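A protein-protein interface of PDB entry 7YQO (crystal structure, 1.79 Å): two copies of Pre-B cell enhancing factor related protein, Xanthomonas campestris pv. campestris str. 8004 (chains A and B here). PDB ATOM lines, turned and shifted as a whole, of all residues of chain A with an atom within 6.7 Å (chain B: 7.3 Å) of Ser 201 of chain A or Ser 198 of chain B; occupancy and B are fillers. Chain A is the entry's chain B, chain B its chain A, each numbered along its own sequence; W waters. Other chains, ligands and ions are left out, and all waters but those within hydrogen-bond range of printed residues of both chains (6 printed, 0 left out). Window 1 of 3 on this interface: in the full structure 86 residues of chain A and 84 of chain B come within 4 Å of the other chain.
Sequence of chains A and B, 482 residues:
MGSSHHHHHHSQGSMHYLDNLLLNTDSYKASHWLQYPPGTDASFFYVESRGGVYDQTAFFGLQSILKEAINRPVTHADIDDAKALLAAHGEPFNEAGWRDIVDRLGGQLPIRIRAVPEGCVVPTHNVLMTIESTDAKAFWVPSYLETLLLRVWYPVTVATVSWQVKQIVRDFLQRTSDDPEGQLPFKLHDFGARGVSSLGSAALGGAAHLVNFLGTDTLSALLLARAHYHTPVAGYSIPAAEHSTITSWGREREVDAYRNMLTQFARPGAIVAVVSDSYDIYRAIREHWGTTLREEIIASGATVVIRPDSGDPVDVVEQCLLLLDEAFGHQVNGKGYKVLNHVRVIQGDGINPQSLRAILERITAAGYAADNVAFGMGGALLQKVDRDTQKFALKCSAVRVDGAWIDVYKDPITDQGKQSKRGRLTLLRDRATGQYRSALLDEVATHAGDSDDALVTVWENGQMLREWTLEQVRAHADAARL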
ATOM      1  N   ARG A 151       3.254  -3.561  24.428  1.00  0.00           N
ATOM      2  CA  ARG A 151       4.703  -3.406  24.570  1.00  0.00           C
ATOM      3  C   ARG A 151       5.093  -2.611  25.814  1.00  0.00           C
ATOM      4  O   ARG A 151       6.289  -2.532  26.118  1.00  0.00           O
ATOM      5  CB  ARG A 151       5.273  -2.764  23.296  1.00  0.00           C
ATOM      6  CG  ARG A 151       5.246  -3.737  22.093  1.00  0.00           C
ATOM      7  CD  ARG A 151       6.198  -3.264  20.969  1.00  0.00           C
ATOM      8  NE  ARG A 151       5.671  -2.061  20.302  1.00  0.00           N
ATOM      9  CZ  ARG A 151       5.151  -2.036  19.074  1.00  0.00           C
ATOM     10  NH1 ARG A 151       5.076  -3.146  18.344  1.00  0.00           N
ATOM     11  NH2 ARG A 151       4.731  -0.885  18.555  1.00  0.00           N
ATOM     12  N   TRP A 153       4.847  -3.955  28.443  1.00  0.00           N
ATOM     13  CA  TRP A 153       5.487  -5.020  29.222  1.00  0.00           C
ATOM     14  C   TRP A 153       6.969  -4.739  29.403  1.00  0.00           C
ATOM     15  O   TRP A 153       7.537  -5.027  30.463  1.00  0.00           O
ATOM     16  CB  TRP A 153       5.271  -6.417  28.583  1.00  0.00           C
ATOM     17  CG  TRP A 153       6.095  -6.680  27.333  1.00  0.00           C
ATOM     18  CD1 TRP A 153       5.657  -6.600  26.039  1.00  0.00           C
ATOM     19  CD2 TRP A 153       7.486  -7.053  27.265  1.00  0.00           C
ATOM     20  NE1 TRP A 153       6.696  -6.877  25.165  1.00  0.00           N
ATOM     21  CE2 TRP A 153       7.826  -7.157  25.893  1.00  0.00           C
ATOM     22  CE3 TRP A 153       8.472  -7.315  28.228  1.00  0.00           C
ATOM     23  CZ2 TRP A 153       9.116  -7.492  25.463  1.00  0.00           C
ATOM     24  CZ3 TRP A 153       9.765  -7.624  27.804  1.00  0.00           C
ATOM     25  CH2 TRP A 153      10.077  -7.712  26.431  1.00  0.00           C
ATOM     26  N   TYR A 154       7.610  -4.140  28.386  1.00  0.00           N
ATOM     27  CA  TYR A 154       9.068  -4.023  28.411  1.00  0.00           C
ATOM     28  C   TYR A 154       9.553  -3.030  29.463  1.00  0.00           C
ATOM     29  O   TYR A 154      10.320  -3.432  30.359  1.00  0.00           O
ATOM     30  CB  TYR A 154       9.586  -3.698  27.009  1.00  0.00           C
ATOM     31  CG  TYR A 154      11.083  -3.475  26.952  1.00  0.00           C
ATOM     32  CD1 TYR A 154      11.969  -4.503  27.279  1.00  0.00           C
ATOM     33  CD2 TYR A 154      11.607  -2.229  26.591  1.00  0.00           C
ATOM     34  CE1 TYR A 154      13.348  -4.303  27.232  1.00  0.00           C
ATOM     35  CE2 TYR A 154      12.980  -2.026  26.512  1.00  0.00           C
ATOM     36  CZ  TYR A 154      13.850  -3.062  26.846  1.00  0.00           C
ATOM     37  OH  TYR A 154      15.222  -2.864  26.793  1.00  0.00           O
ATOM     38  N   VAL A 196      21.208  -4.646  23.391  1.00  0.00           N
ATOM     39  CA  VAL A 196      19.763  -4.578  23.248  1.00  0.00           C
ATOM     40  C   VAL A 196      19.435  -4.509  21.757  1.00  0.00           C
ATOM     41  O   VAL A 196      20.295  -4.227  20.913  1.00  0.00           O
ATOM     42  CB  VAL A 196      19.197  -3.376  24.047  1.00  0.00           C
ATOM     43  CG1 VAL A 196      19.627  -2.063  23.427  1.00  0.00           C
ATOM     44  CG2 VAL A 196      17.652  -3.470  24.229  1.00  0.00           C
ATOM     45  N   SER A 197      18.180  -4.792  21.420  1.00  0.00           N
ATOM     46  CA  SER A 197      17.837  -5.064  20.021  1.00  0.00           C
ATOM     47  C   SER A 197      17.673  -3.813  19.148  1.00  0.00           C
ATOM     48  O   SER A 197      17.744  -3.938  17.923  1.00  0.00           O
ATOM     49  CB  SER A 197      16.561  -5.914  19.965  1.00  0.00           C
ATOM     50  OG  SER A 197      15.496  -5.282  20.688  1.00  0.00           O
ATOM     51  N   SER A 198      17.458  -2.620  19.709  1.00  0.00           N
ATOM     52  CA  SER A 198      17.395  -1.421  18.872  1.00  0.00           C
ATOM     53  C   SER A 198      17.643  -0.196  19.733  1.00  0.00           C
ATOM     54  O   SER A 198      17.588  -0.251  20.965  1.00  0.00           O
ATOM     55  CB  SER A 198      16.040  -1.274  18.160  1.00  0.00           C
ATOM     56  OG  SER A 198      14.990  -1.069  19.114  1.00  0.00           O
ATOM     57  N   LEU A 199      17.879   0.918  19.044  1.00  0.00           N
ATOM     58  CA  LEU A 199      18.025   2.226  19.684  1.00  0.00           C
ATOM     59  C   LEU A 199      16.819   2.568  20.554  1.00  0.00           C
ATOM     60  O   LEU A 199      16.969   3.034  21.690  1.00  0.00           O
ATOM     61  CB  LEU A 199      18.212   3.293  18.603  1.00  0.00           C
ATOM     62  CG  LEU A 199      18.216   4.760  19.027  1.00  0.00           C
ATOM     63  CD1 LEU A 199      19.334   4.968  20.059  1.00  0.00           C
ATOM     64  CD2 LEU A 199      18.417   5.636  17.781  1.00  0.00           C
ATOM     65  N   GLY A 200      15.611   2.337  20.033  1.00  0.00           N
ATOM     66  CA  GLY A 200      14.413   2.673  20.790  1.00  0.00           C
ATOM     67  C   GLY A 200      14.278   1.853  22.057  1.00  0.00           C
ATOM     68  O   GLY A 200      13.835   2.353  23.092  1.00  0.00           O
ATOM     69  N   SER A 201      14.619   0.566  21.981  1.00  0.00           N
ATOM     70  CA  SER A 201      14.612  -0.261  23.181  1.00  0.00           C
ATOM     71  C   SER A 201      15.698   0.177  24.172  1.00  0.00           C
ATOM     72  O   SER A 201      15.466   0.182  25.389  1.00  0.00           O
ATOM     73  CB  SER A 201      14.778  -1.729  22.781  1.00  0.00           C
ATOM     74  OG  SER A 201      13.646  -2.182  22.014  1.00  0.00           O
ATOM     75  N   ALA A 202      16.891   0.538  23.676  1.00  0.00           N
ATOM     76  CA  ALA A 202      17.921   1.076  24.576  1.00  0.00           C
ATOM     77  C   ALA A 202      17.411   2.310  25.310  1.00  0.00           C
ATOM     78  O   ALA A 202      17.636   2.459  26.517  1.00  0.00           O
ATOM     79  CB  ALA A 202      19.187   1.442  23.797  1.00  0.00           C
ATOM     80  N   ALA A 203      16.741   3.220  24.595  1.00  0.00           N
ATOM     81  CA  ALA A 203      16.250   4.442  25.232  1.00  0.00           C
ATOM     82  C   ALA A 203      15.197   4.141  26.302  1.00  0.00           C
ATOM     83  O   ALA A 203      15.257   4.682  27.411  1.00  0.00           O
ATOM     84  CB  ALA A 203      15.679   5.386  24.172  1.00  0.00           C
ATOM     85  N   LEU A 204      14.203   3.303  25.973  1.00  0.00           N
ATOM     86  CA  LEU A 204      13.076   3.093  26.885  1.00  0.00           C
ATOM     87  C   LEU A 204      13.454   2.145  28.012  1.00  0.00           C
ATOM     88  O   LEU A 204      13.106   2.389  29.176  1.00  0.00           O
ATOM     89  CB  LEU A 204      11.862   2.552  26.114  1.00  0.00           C
ATOM     90  CG  LEU A 204      10.560   2.391  26.902  1.00  0.00           C
ATOM     91  CD1 LEU A 204      10.201   3.655  27.689  1.00  0.00           C
ATOM     92  CD2 LEU A 204       9.436   2.002  25.959  1.00  0.00           C
ATOM     93  N   GLY A 205      14.180   1.074  27.693  1.00  0.00           N
ATOM     94  CA  GLY A 205      14.657   0.183  28.741  1.00  0.00           C
ATOM     95  C   GLY A 205      15.688   0.855  29.624  1.00  0.00           C
ATOM     96  O   GLY A 205      15.666   0.704  30.849  1.00  0.00           O
ATOM     97  N   GLY A 206      16.589   1.628  29.019  1.00  0.00           N
ATOM     98  CA  GLY A 206      17.552   2.368  29.817  1.00  0.00           C
ATOM     99  C   GLY A 206      16.875   3.354  30.754  1.00  0.00           C
ATOM    100  O   GLY A 206      17.294   3.537  31.898  1.00  0.00           O
ATOM    101  N   ALA A 207      15.807   3.992  30.289  1.00  0.00           N
ATOM    102  CA  ALA A 207      15.103   4.931  31.154  1.00  0.00           C
ATOM    103  C   ALA A 207      14.390   4.207  32.291  1.00  0.00           C
ATOM    104  O   ALA A 207      14.310   4.739  33.410  1.00  0.00           O
ATOM    105  CB  ALA A 207      14.113   5.758  30.330  1.00  0.00           C
ATOM    106  N   THR A 218      23.953   4.287  29.039  1.00  0.00           N
ATOM    107  CA  THR A 218      23.037   4.309  27.905  1.00  0.00           C
ATOM    108  C   THR A 218      22.594   5.750  27.664  1.00  0.00           C
ATOM    109  O   THR A 218      21.612   6.226  28.233  1.00  0.00           O
ATOM    110  CB  THR A 218      21.868   3.369  28.185  1.00  0.00           C
ATOM    111  OG1 THR A 218      22.392   2.048  28.414  1.00  0.00           O
ATOM    112  CG2 THR A 218      20.900   3.334  27.006  1.00  0.00           C
ATOM    113  N   LEU A 382      18.619  -5.241  29.831  1.00  0.00           N
ATOM    114  CA  LEU A 382      17.827  -4.631  28.770  1.00  0.00           C
ATOM    115  C   LEU A 382      17.285  -5.616  27.752  1.00  0.00           C
ATOM    116  O   LEU A 382      16.335  -5.267  27.039  1.00  0.00           O
ATOM    117  CB  LEU A 382      18.643  -3.581  28.003  1.00  0.00           C
ATOM    118  CG  LEU A 382      19.216  -2.426  28.817  1.00  0.00           C
ATOM    119  CD1 LEU A 382      19.794  -1.411  27.851  1.00  0.00           C
ATOM    120  CD2 LEU A 382      18.095  -1.826  29.695  1.00  0.00           C
ATOM    121  N   GLN A 383      17.867  -6.814  27.642  1.00  0.00           N
ATOM    122  CA  GLN A 383      17.509  -7.705  26.539  1.00  0.00           C
ATOM    123  C   GLN A 383      17.007  -9.064  26.990  1.00  0.00           C
ATOM    124  O   GLN A 383      16.104  -9.623  26.359  1.00  0.00           O
ATOM    125  CB  GLN A 383      18.728  -7.887  25.606  1.00  0.00           C
ATOM    126  CG  GLN A 383      18.422  -8.686  24.324  1.00  0.00           C
ATOM    127  CD  GLN A 383      17.291  -8.073  23.505  1.00  0.00           C
ATOM    128  OE1 GLN A 383      17.183  -6.855  23.403  1.00  0.00           O
ATOM    129  NE2 GLN A 383      16.456  -8.925  22.904  1.00  0.00           N
ATOM    130  N   MET B  15      10.656  10.355  16.584  1.00  0.00           N
ATOM    131  CA  MET B  15      11.940   9.857  17.076  1.00  0.00           C
ATOM    132  C   MET B  15      12.972  10.970  17.062  1.00  0.00           C
ATOM    133  O   MET B  15      14.164  10.721  17.295  1.00  0.00           O
ATOM    134  CB  MET B  15      12.427   8.670  16.234  1.00  0.00           C
ATOM    135  CG  MET B  15      11.648   7.382  16.463  1.00  0.00           C
ATOM    136  SD  MET B  15      12.449   5.929  15.733  1.00  0.00           S
ATOM    137  CE  MET B  15      13.556   5.427  17.068  1.00  0.00           C
ATOM    138  N   LEU B  18      15.847  11.419  19.461  1.00  0.00           N
ATOM    139  CA  LEU B  18      17.009  10.549  19.344  1.00  0.00           C
ATOM    140  C   LEU B  18      17.867  10.891  18.126  1.00  0.00           C
ATOM    141  O   LEU B  18      18.780  10.135  17.785  1.00  0.00           O
ATOM    142  CB  LEU B  18      16.559   9.082  19.276  1.00  0.00           C
ATOM    143  CG  LEU B  18      15.947   8.466  20.542  1.00  0.00           C
ATOM    144  CD1 LEU B  18      15.398   7.056  20.292  1.00  0.00           C
ATOM    145  CD2 LEU B  18      16.938   8.446  21.703  1.00  0.00           C
ATOM    146  N   ARG B 151      24.775  -3.729  17.445  1.00  0.00           N
ATOM    147  CA  ARG B 151      23.368  -4.145  17.478  1.00  0.00           C
ATOM    148  C   ARG B 151      22.925  -4.871  16.200  1.00  0.00           C
ATOM    149  O   ARG B 151      21.804  -5.390  16.157  1.00  0.00           O
ATOM    150  CB  ARG B 151      22.482  -2.928  17.780  1.00  0.00           C
ATOM    151  CG  ARG B 151      22.605  -2.512  19.263  1.00  0.00           C
ATOM    152  CD  ARG B 151      21.478  -1.567  19.691  1.00  0.00           C
ATOM    153  NE  ARG B 151      21.536  -0.277  18.994  1.00  0.00           N
ATOM    154  CZ  ARG B 151      21.817   0.900  19.560  1.00  0.00           C
ATOM    155  NH1 ARG B 151      22.112   0.993  20.853  1.00  0.00           N
ATOM    156  NH2 ARG B 151      21.809   1.999  18.821  1.00  0.00           N
ATOM    157  N   TYR B 154      21.219  -8.349  16.399  1.00  0.00           N
ATOM    158  CA  TYR B 154      19.790  -8.644  16.497  1.00  0.00           C
ATOM    159  C   TYR B 154      19.213  -9.098  15.157  1.00  0.00           C
ATOM    160  O   TYR B 154      18.701 -10.224  15.079  1.00  0.00           O
ATOM    161  CB  TYR B 154      19.049  -7.441  17.098  1.00  0.00           C
ATOM    162  CG  TYR B 154      17.547  -7.657  17.163  1.00  0.00           C
ATOM    163  CD1 TYR B 154      17.018  -8.682  17.923  1.00  0.00           C
ATOM    164  CD2 TYR B 154      16.675  -6.842  16.437  1.00  0.00           C
ATOM    165  CE1 TYR B 154      15.640  -8.910  17.977  1.00  0.00           C
ATOM    166  CE2 TYR B 154      15.287  -7.048  16.479  1.00  0.00           C
ATOM    167  CZ  TYR B 154      14.787  -8.099  17.253  1.00  0.00           C
ATOM    168  OH  TYR B 154      13.437  -8.317  17.322  1.00  0.00           O
ATOM    169  N   GLY B 192       4.948 -11.497  16.337  1.00  0.00           N
ATOM    170  CA  GLY B 192       5.637 -11.049  17.536  1.00  0.00           C
ATOM    171  C   GLY B 192       5.624  -9.568  17.848  1.00  0.00           C
ATOM    172  O   GLY B 192       6.325  -9.149  18.780  1.00  0.00           O
ATOM    173  N   ALA B 193       4.862  -8.751  17.119  1.00  0.00           N
ATOM    174  CA  ALA B 193       4.965  -7.312  17.343  1.00  0.00           C
ATOM    175  C   ALA B 193       4.541  -6.918  18.760  1.00  0.00           C
ATOM    176  O   ALA B 193       5.079  -5.954  19.314  1.00  0.00           O
ATOM    177  CB  ALA B 193       4.135  -6.551  16.308  1.00  0.00           C
ATOM    178  N   GLY B 195       5.000  -8.790  21.434  1.00  0.00           N
ATOM    179  CA  GLY B 195       5.936  -9.418  22.347  1.00  0.00           C
ATOM    180  C   GLY B 195       7.370  -8.924  22.271  1.00  0.00           C
ATOM    181  O   GLY B 195       8.232  -9.489  22.949  1.00  0.00           O
ATOM    182  N   VAL B 196       7.659  -7.910  21.467  1.00  0.00           N
ATOM    183  CA  VAL B 196       9.012  -7.394  21.311  1.00  0.00           C
ATOM    184  C   VAL B 196       9.104  -6.053  22.050  1.00  0.00           C
ATOM    185  O   VAL B 196       8.100  -5.464  22.430  1.00  0.00           O
ATOM    186  CB  VAL B 196       9.396  -7.291  19.814  1.00  0.00           C
ATOM    187  CG1 VAL B 196       8.608  -6.183  19.135  1.00  0.00           C
ATOM    188  CG2 VAL B 196      10.927  -7.154  19.594  1.00  0.00           C
ATOM    189  N   SER B 197      10.337  -5.567  22.261  1.00  0.00           N
ATOM    190  CA  SER B 197      10.538  -4.494  23.236  1.00  0.00           C
ATOM    191  C   SER B 197      10.273  -3.092  22.686  1.00  0.00           C
ATOM    192  O   SER B 197      10.072  -2.167  23.485  1.00  0.00           O
ATOM    193  CB  SER B 197      11.970  -4.571  23.811  1.00  0.00           C
ATOM    194  OG  SER B 197      12.941  -4.581  22.787  1.00  0.00           O
ATOM    195  N   SER B 198      10.263  -2.907  21.365  1.00  0.00           N
ATOM    196  CA  SER B 198      10.112  -1.592  20.742  1.00  0.00           C
ATOM    197  C   SER B 198       9.522  -1.757  19.353  1.00  0.00           C
ATOM    198  O   SER B 198       9.692  -2.791  18.705  1.00  0.00           O
ATOM    199  CB  SER B 198      11.469  -0.843  20.577  1.00  0.00           C
ATOM    200  N   LEU B 199       8.878  -0.681  18.880  1.00  0.00           N
ATOM    201  CA  LEU B 199       8.471  -0.580  17.475  1.00  0.00           C
ATOM    202  C   LEU B 199       9.659  -0.788  16.526  1.00  0.00           C
ATOM    203  O   LEU B 199       9.564  -1.516  15.532  1.00  0.00           O
ATOM    204  CB  LEU B 199       7.843   0.802  17.240  1.00  0.00           C
ATOM    205  CG  LEU B 199       7.509   1.251  15.804  1.00  0.00           C
ATOM    206  CD1 LEU B 199       6.629   0.209  15.095  1.00  0.00           C
ATOM    207  CD2 LEU B 199       6.837   2.623  15.829  1.00  0.00           C
ATOM    208  N   GLY B 200      10.792  -0.146  16.819  1.00  0.00           N
ATOM    209  CA  GLY B 200      11.954  -0.294  15.950  1.00  0.00           C
ATOM    210  C   GLY B 200      12.475  -1.714  15.934  1.00  0.00           C
ATOM    211  O   GLY B 200      12.926  -2.214  14.897  1.00  0.00           O
ATOM    212  N   SER B 201      12.405  -2.393  17.080  1.00  0.00           N
ATOM    213  CA  SER B 201      12.780  -3.801  17.119  1.00  0.00           C
ATOM    214  C   SER B 201      11.786  -4.661  16.347  1.00  0.00           C
ATOM    215  O   SER B 201      12.178  -5.629  15.680  1.00  0.00           O
ATOM    216  CB  SER B 201      12.913  -4.242  18.579  1.00  0.00           C
ATOM    217  OG  SER B 201      14.053  -3.583  19.151  1.00  0.00           O
ATOM    218  N   ALA B 202      10.488  -4.357  16.456  1.00  0.00           N
ATOM    219  CA  ALA B 202       9.504  -5.095  15.660  1.00  0.00           C
ATOM    220  C   ALA B 202       9.788  -4.948  14.168  1.00  0.00           C
ATOM    221  O   ALA B 202       9.704  -5.924  13.410  1.00  0.00           O
ATOM    222  CB  ALA B 202       8.091  -4.598  15.980  1.00  0.00           C
ATOM    223  N   ALA B 203      10.139  -3.740  13.733  1.00  0.00           N
ATOM    224  CA  ALA B 203      10.353  -3.502  12.307  1.00  0.00           C
ATOM    225  C   ALA B 203      11.583  -4.257  11.804  1.00  0.00           C
ATOM    226  O   ALA B 203      11.531  -4.936  10.776  1.00  0.00           O
ATOM    227  CB  ALA B 203      10.496  -2.003  12.053  1.00  0.00           C
ATOM    228  N   LEU B 204      12.702  -4.149  12.523  1.00  0.00           N
ATOM    229  CA  LEU B 204      13.941  -4.771  12.060  1.00  0.00           C
ATOM    230  C   LEU B 204      13.923  -6.280  12.274  1.00  0.00           C
ATOM    231  O   LEU B 204      14.323  -7.047  11.386  1.00  0.00           O
ATOM    232  CB  LEU B 204      15.133  -4.135  12.784  1.00  0.00           C
ATOM    233  CG  LEU B 204      16.548  -4.540  12.372  1.00  0.00           C
ATOM    234  CD1 LEU B 204      16.745  -4.458  10.881  1.00  0.00           C
ATOM    235  CD2 LEU B 204      17.561  -3.647  13.102  1.00  0.00           C
ATOM    236  N   SER B 220       5.013  -3.319  10.743  1.00  0.00           N
ATOM    237  CA  SER B 220       6.240  -2.513  10.787  1.00  0.00           C
ATOM    238  C   SER B 220       7.353  -3.100   9.922  1.00  0.00           C
ATOM    239  O   SER B 220       8.187  -2.350   9.405  1.00  0.00           O
ATOM    240  CB  SER B 220       6.743  -2.362  12.233  1.00  0.00           C
ATOM    241  OG  SER B 220       5.672  -2.045  13.105  1.00  0.00           O
ATOM    242  N   LEU B 382      11.142 -12.823  18.004  1.00  0.00           N
ATOM    243  CA  LEU B 382      11.624 -11.449  17.979  1.00  0.00           C
ATOM    244  C   LEU B 382      12.260 -10.992  19.274  1.00  0.00           C
ATOM    245  O   LEU B 382      12.964  -9.973  19.260  1.00  0.00           O
ATOM    246  CB  LEU B 382      10.477 -10.478  17.679  1.00  0.00           C
ATOM    247  CG  LEU B 382       9.763 -10.626  16.327  1.00  0.00           C
ATOM    248  CD1 LEU B 382       8.890  -9.400  16.124  1.00  0.00           C
ATOM    249  CD2 LEU B 382      10.777 -10.760  15.175  1.00  0.00           C
ATOM    250  N   GLN B 383      11.991 -11.671  20.393  1.00  0.00           N
ATOM    251  CA  GLN B 383      12.416 -11.154  21.691  1.00  0.00           C
ATOM    252  C   GLN B 383      13.283 -12.107  22.496  1.00  0.00           C
ATOM    253  O   GLN B 383      14.185 -11.638  23.202  1.00  0.00           O
ATOM    254  CB  GLN B 383      11.189 -10.763  22.531  1.00  0.00           C
ATOM    255  CG  GLN B 383      11.520 -10.084  23.876  1.00  0.00           C
ATOM    256  CD  GLN B 383      12.291  -8.790  23.705  1.00  0.00           C
ATOM    257  OE1 GLN B 383      12.071  -8.039  22.754  1.00  0.00           O
ATOM    258  NE2 GLN B 383      13.200  -8.511  24.654  1.00  0.00           N
HETATM  259  O   HOH W   1       8.129  -0.858  24.881  1.00  0.00           O
HETATM  260  O   HOH W   2      14.226  -7.746  21.188  1.00  0.00           O
HETATM  261  O   HOH W   3      19.497  -3.977  15.808  1.00  0.00           O
HETATM  262  O   HOH W   4       4.239  -2.616  15.485  1.00  0.00           O
HETATM  263  O   HOH W   5      15.400 -12.124  25.596  1.00  0.00           O
HETATM  264  O   HOH W   6      14.912  -5.927  24.335  1.00  0.00           O
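The guanidinium group (NH1) of Arg 151 of chain A sits at hydrogen-bond distance from the backbone carbonyl oxygen (O) of Ala 193 of chain B, at 3.0 Å. The backbone carbonyl oxygen (O) of Val 196 of chain B lies within hydrogen-bond range of the indole nitrogen (NE1) of Trp 153 of chain A (3.4 Å). OG of Ser 197 of chain B lies within hydrogen-bond range of OG of Ser 197 of chain A, at 3.4 Å. The side-chain hydroxyl of Ser 197 of chain B lies within hydrogen-bond range of the side-chain hydroxyl of Ser 201 of chain A, at 2.6 Å. The side-chain hydroxyl of Ser 201 of chain B is in hydrogen-bond range of the side-chain hydroxyl of Ser 197 of chain A (2.7 Å). The side-chain hydroxyl (OG) of Ser 201 of chain B lies within hydrogen-bond range of the side-chain hydroxyl (OG) of Ser 198 of chain A (2.7 Å). OG of Ser 201 of chain B sits at hydrogen-bond distance from OG of Ser 201 of chain A, at 3.2 Å.
The side-chain hydroxyl of Tyr 154 of chain B lies within hydrogen-bond range of the backbone carbonyl oxygen of Ser 201 of chain B, 3.4 Å away. The backbone carbonyl oxygen (O) of Leu 382 of chain B sits at hydrogen-bond distance from the side-chain hydroxyl (OH) of Tyr 154 of chain B, 2.6 Å away. The side-chain amide oxygen (OE1) of Gln 383 of chain B is in hydrogen-bond range of the backbone NH (N) of Ser 197 of chain B (3.1 Å). The backbone carbonyl oxygen (O) of Leu 382 of chain A sits at hydrogen-bond distance from the side-chain hydroxyl (OH) of Tyr 154 of chain A (2.7 Å). N of Ser 197 of chain A sits at hydrogen-bond distance from OE1 of Gln 383 of chain A (3.0 Å). OG of Ser 198 of chain A sits at hydrogen-bond distance from N of Ser 201 of chain A (3.3 Å).
Among the printed residues, pairs that only touch across the chains: Arg 151 of chain A with Val 196 of chain B, Arg 151 of chain A with Ser 198 of chain B, Arg 151 of chain A with Leu 199 of chain B, Trp 153 of chain A with Gly 195 of chain B, Trp 153 of chain A with Ser 197 of chain B, Trp 153 of chain A with Gln 383 of chain B, Tyr 154 of chain A with Ser 197 of chain B, Val 196 of chain A with Arg 151 of chain B, Ser 197 of chain A with Tyr 154 of chain B, Ser 198 of chain A with Arg 151 of chain B, Ser 198 of chain A with Ser 198 of chain B, Leu 199 of chain A with Leu 18 of chain B, Leu 199 of chain A with Arg 151 of chain B, Ser 201 of chain A with Ser 198 of chain B and Gln 383 of chain A with Gln 383 of chain B.
Printed residues of chain B within 4 Å of Trp 153 of chain A: Gly 195, Val 196, Ser 197 and Gln 383. Printed residues of chain B within 4 Å of Val 196 of chain A: Arg 151 (3.2 Å). No residue of chain B comes within 4 Å of Gly 200 of chain A. Of the printed residues of chain A, Gly 195 of chain B touches Trp 153 (3.3 Å). Printed residues of chain A within 4 Å of Val 196 of chain B: Arg 151 and Trp 153. Of the printed residues of chain A, Ser 197 of chain B touches Trp 153 (3.9 Å), Tyr 154 (3.4 Å), Ser 197 (3.4 Å) and Ser 201 (2.6 Å). Of chain A, only Arg 151 (3.98 Å), Ser 198 (3.8 Å) and Ser 201 (2.9 Å) come within 4 Å of Ser 198 of chain B. The nearest residue of chain B that does not touch Ser 201 of chain A is Leu 199 of chain B (5.9 Å).
Hydrophobic or aromatic side chains of chain A within 4 Å of the printed part of chain B: Trp 153, Tyr 154 and Leu 199. Printed residues of chain B that touch a printed residue of chain A: Leu 18, Arg 151, Tyr 154, Ala 193, Gly 195, Val 196, Ser 197, Ser 198, Leu 199, Ser 201 and Gln 383.
Arg 151 of chain A touches Leu 199 of chain B, and with the chains exchanged Leu 199 of chain A touches Arg 151 of chain B. Tyr 154 of chain A touches Ser 197 of chain B, and with the chains exchanged Ser 197 of chain A touches Tyr 154 of chain B. Ser 197 of chain B touches its own counterpart, Ser 197 of chain A. Ser 198 of chain A touches Ser 201 of chain B, and with the chains exchanged Ser 201 of chain A touches Ser 198 of chain B.
Water W6 lies within hydrogen-bond range of OE1 of Gln 383 of chain A (2.6 Å), OG of Ser 197 of chain B (2.8 Å), NE2 of Gln 383 of chain B (3.1 Å) and O of Leu 382 of chain A (3.1 Å). Water W2 lies within hydrogen-bond range of OE1 of Gln 383 of chain B (2.7 Å), OG of Ser 197 of chain A (2.8 Å), NE2 of Gln 383 of chain A (3.1 Å) and O of Leu 382 of chain B (3.2 Å). Water W5 lies within hydrogen-bond range of O of Gln 383 of chain A (2.7 Å) and O of Gln 383 of chain B (2.7 Å). Water W1 bridges the backbone carbonyl oxygen (O) of Ser 197 of chain B (2.7 Å) and the backbone carbonyl oxygen (O) of Arg 151 of chain A (2.8 Å). Water W3 lies within hydrogen-bond range of the backbone carbonyl oxygen (O) of Arg 151 of chain B and the backbone carbonyl oxygen (O) of Ser 197 of chain A. Water W4 bridges the side-chain hydroxyl of Ser 220 of chain B and the guanidinium group of Arg 151 of chain A.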
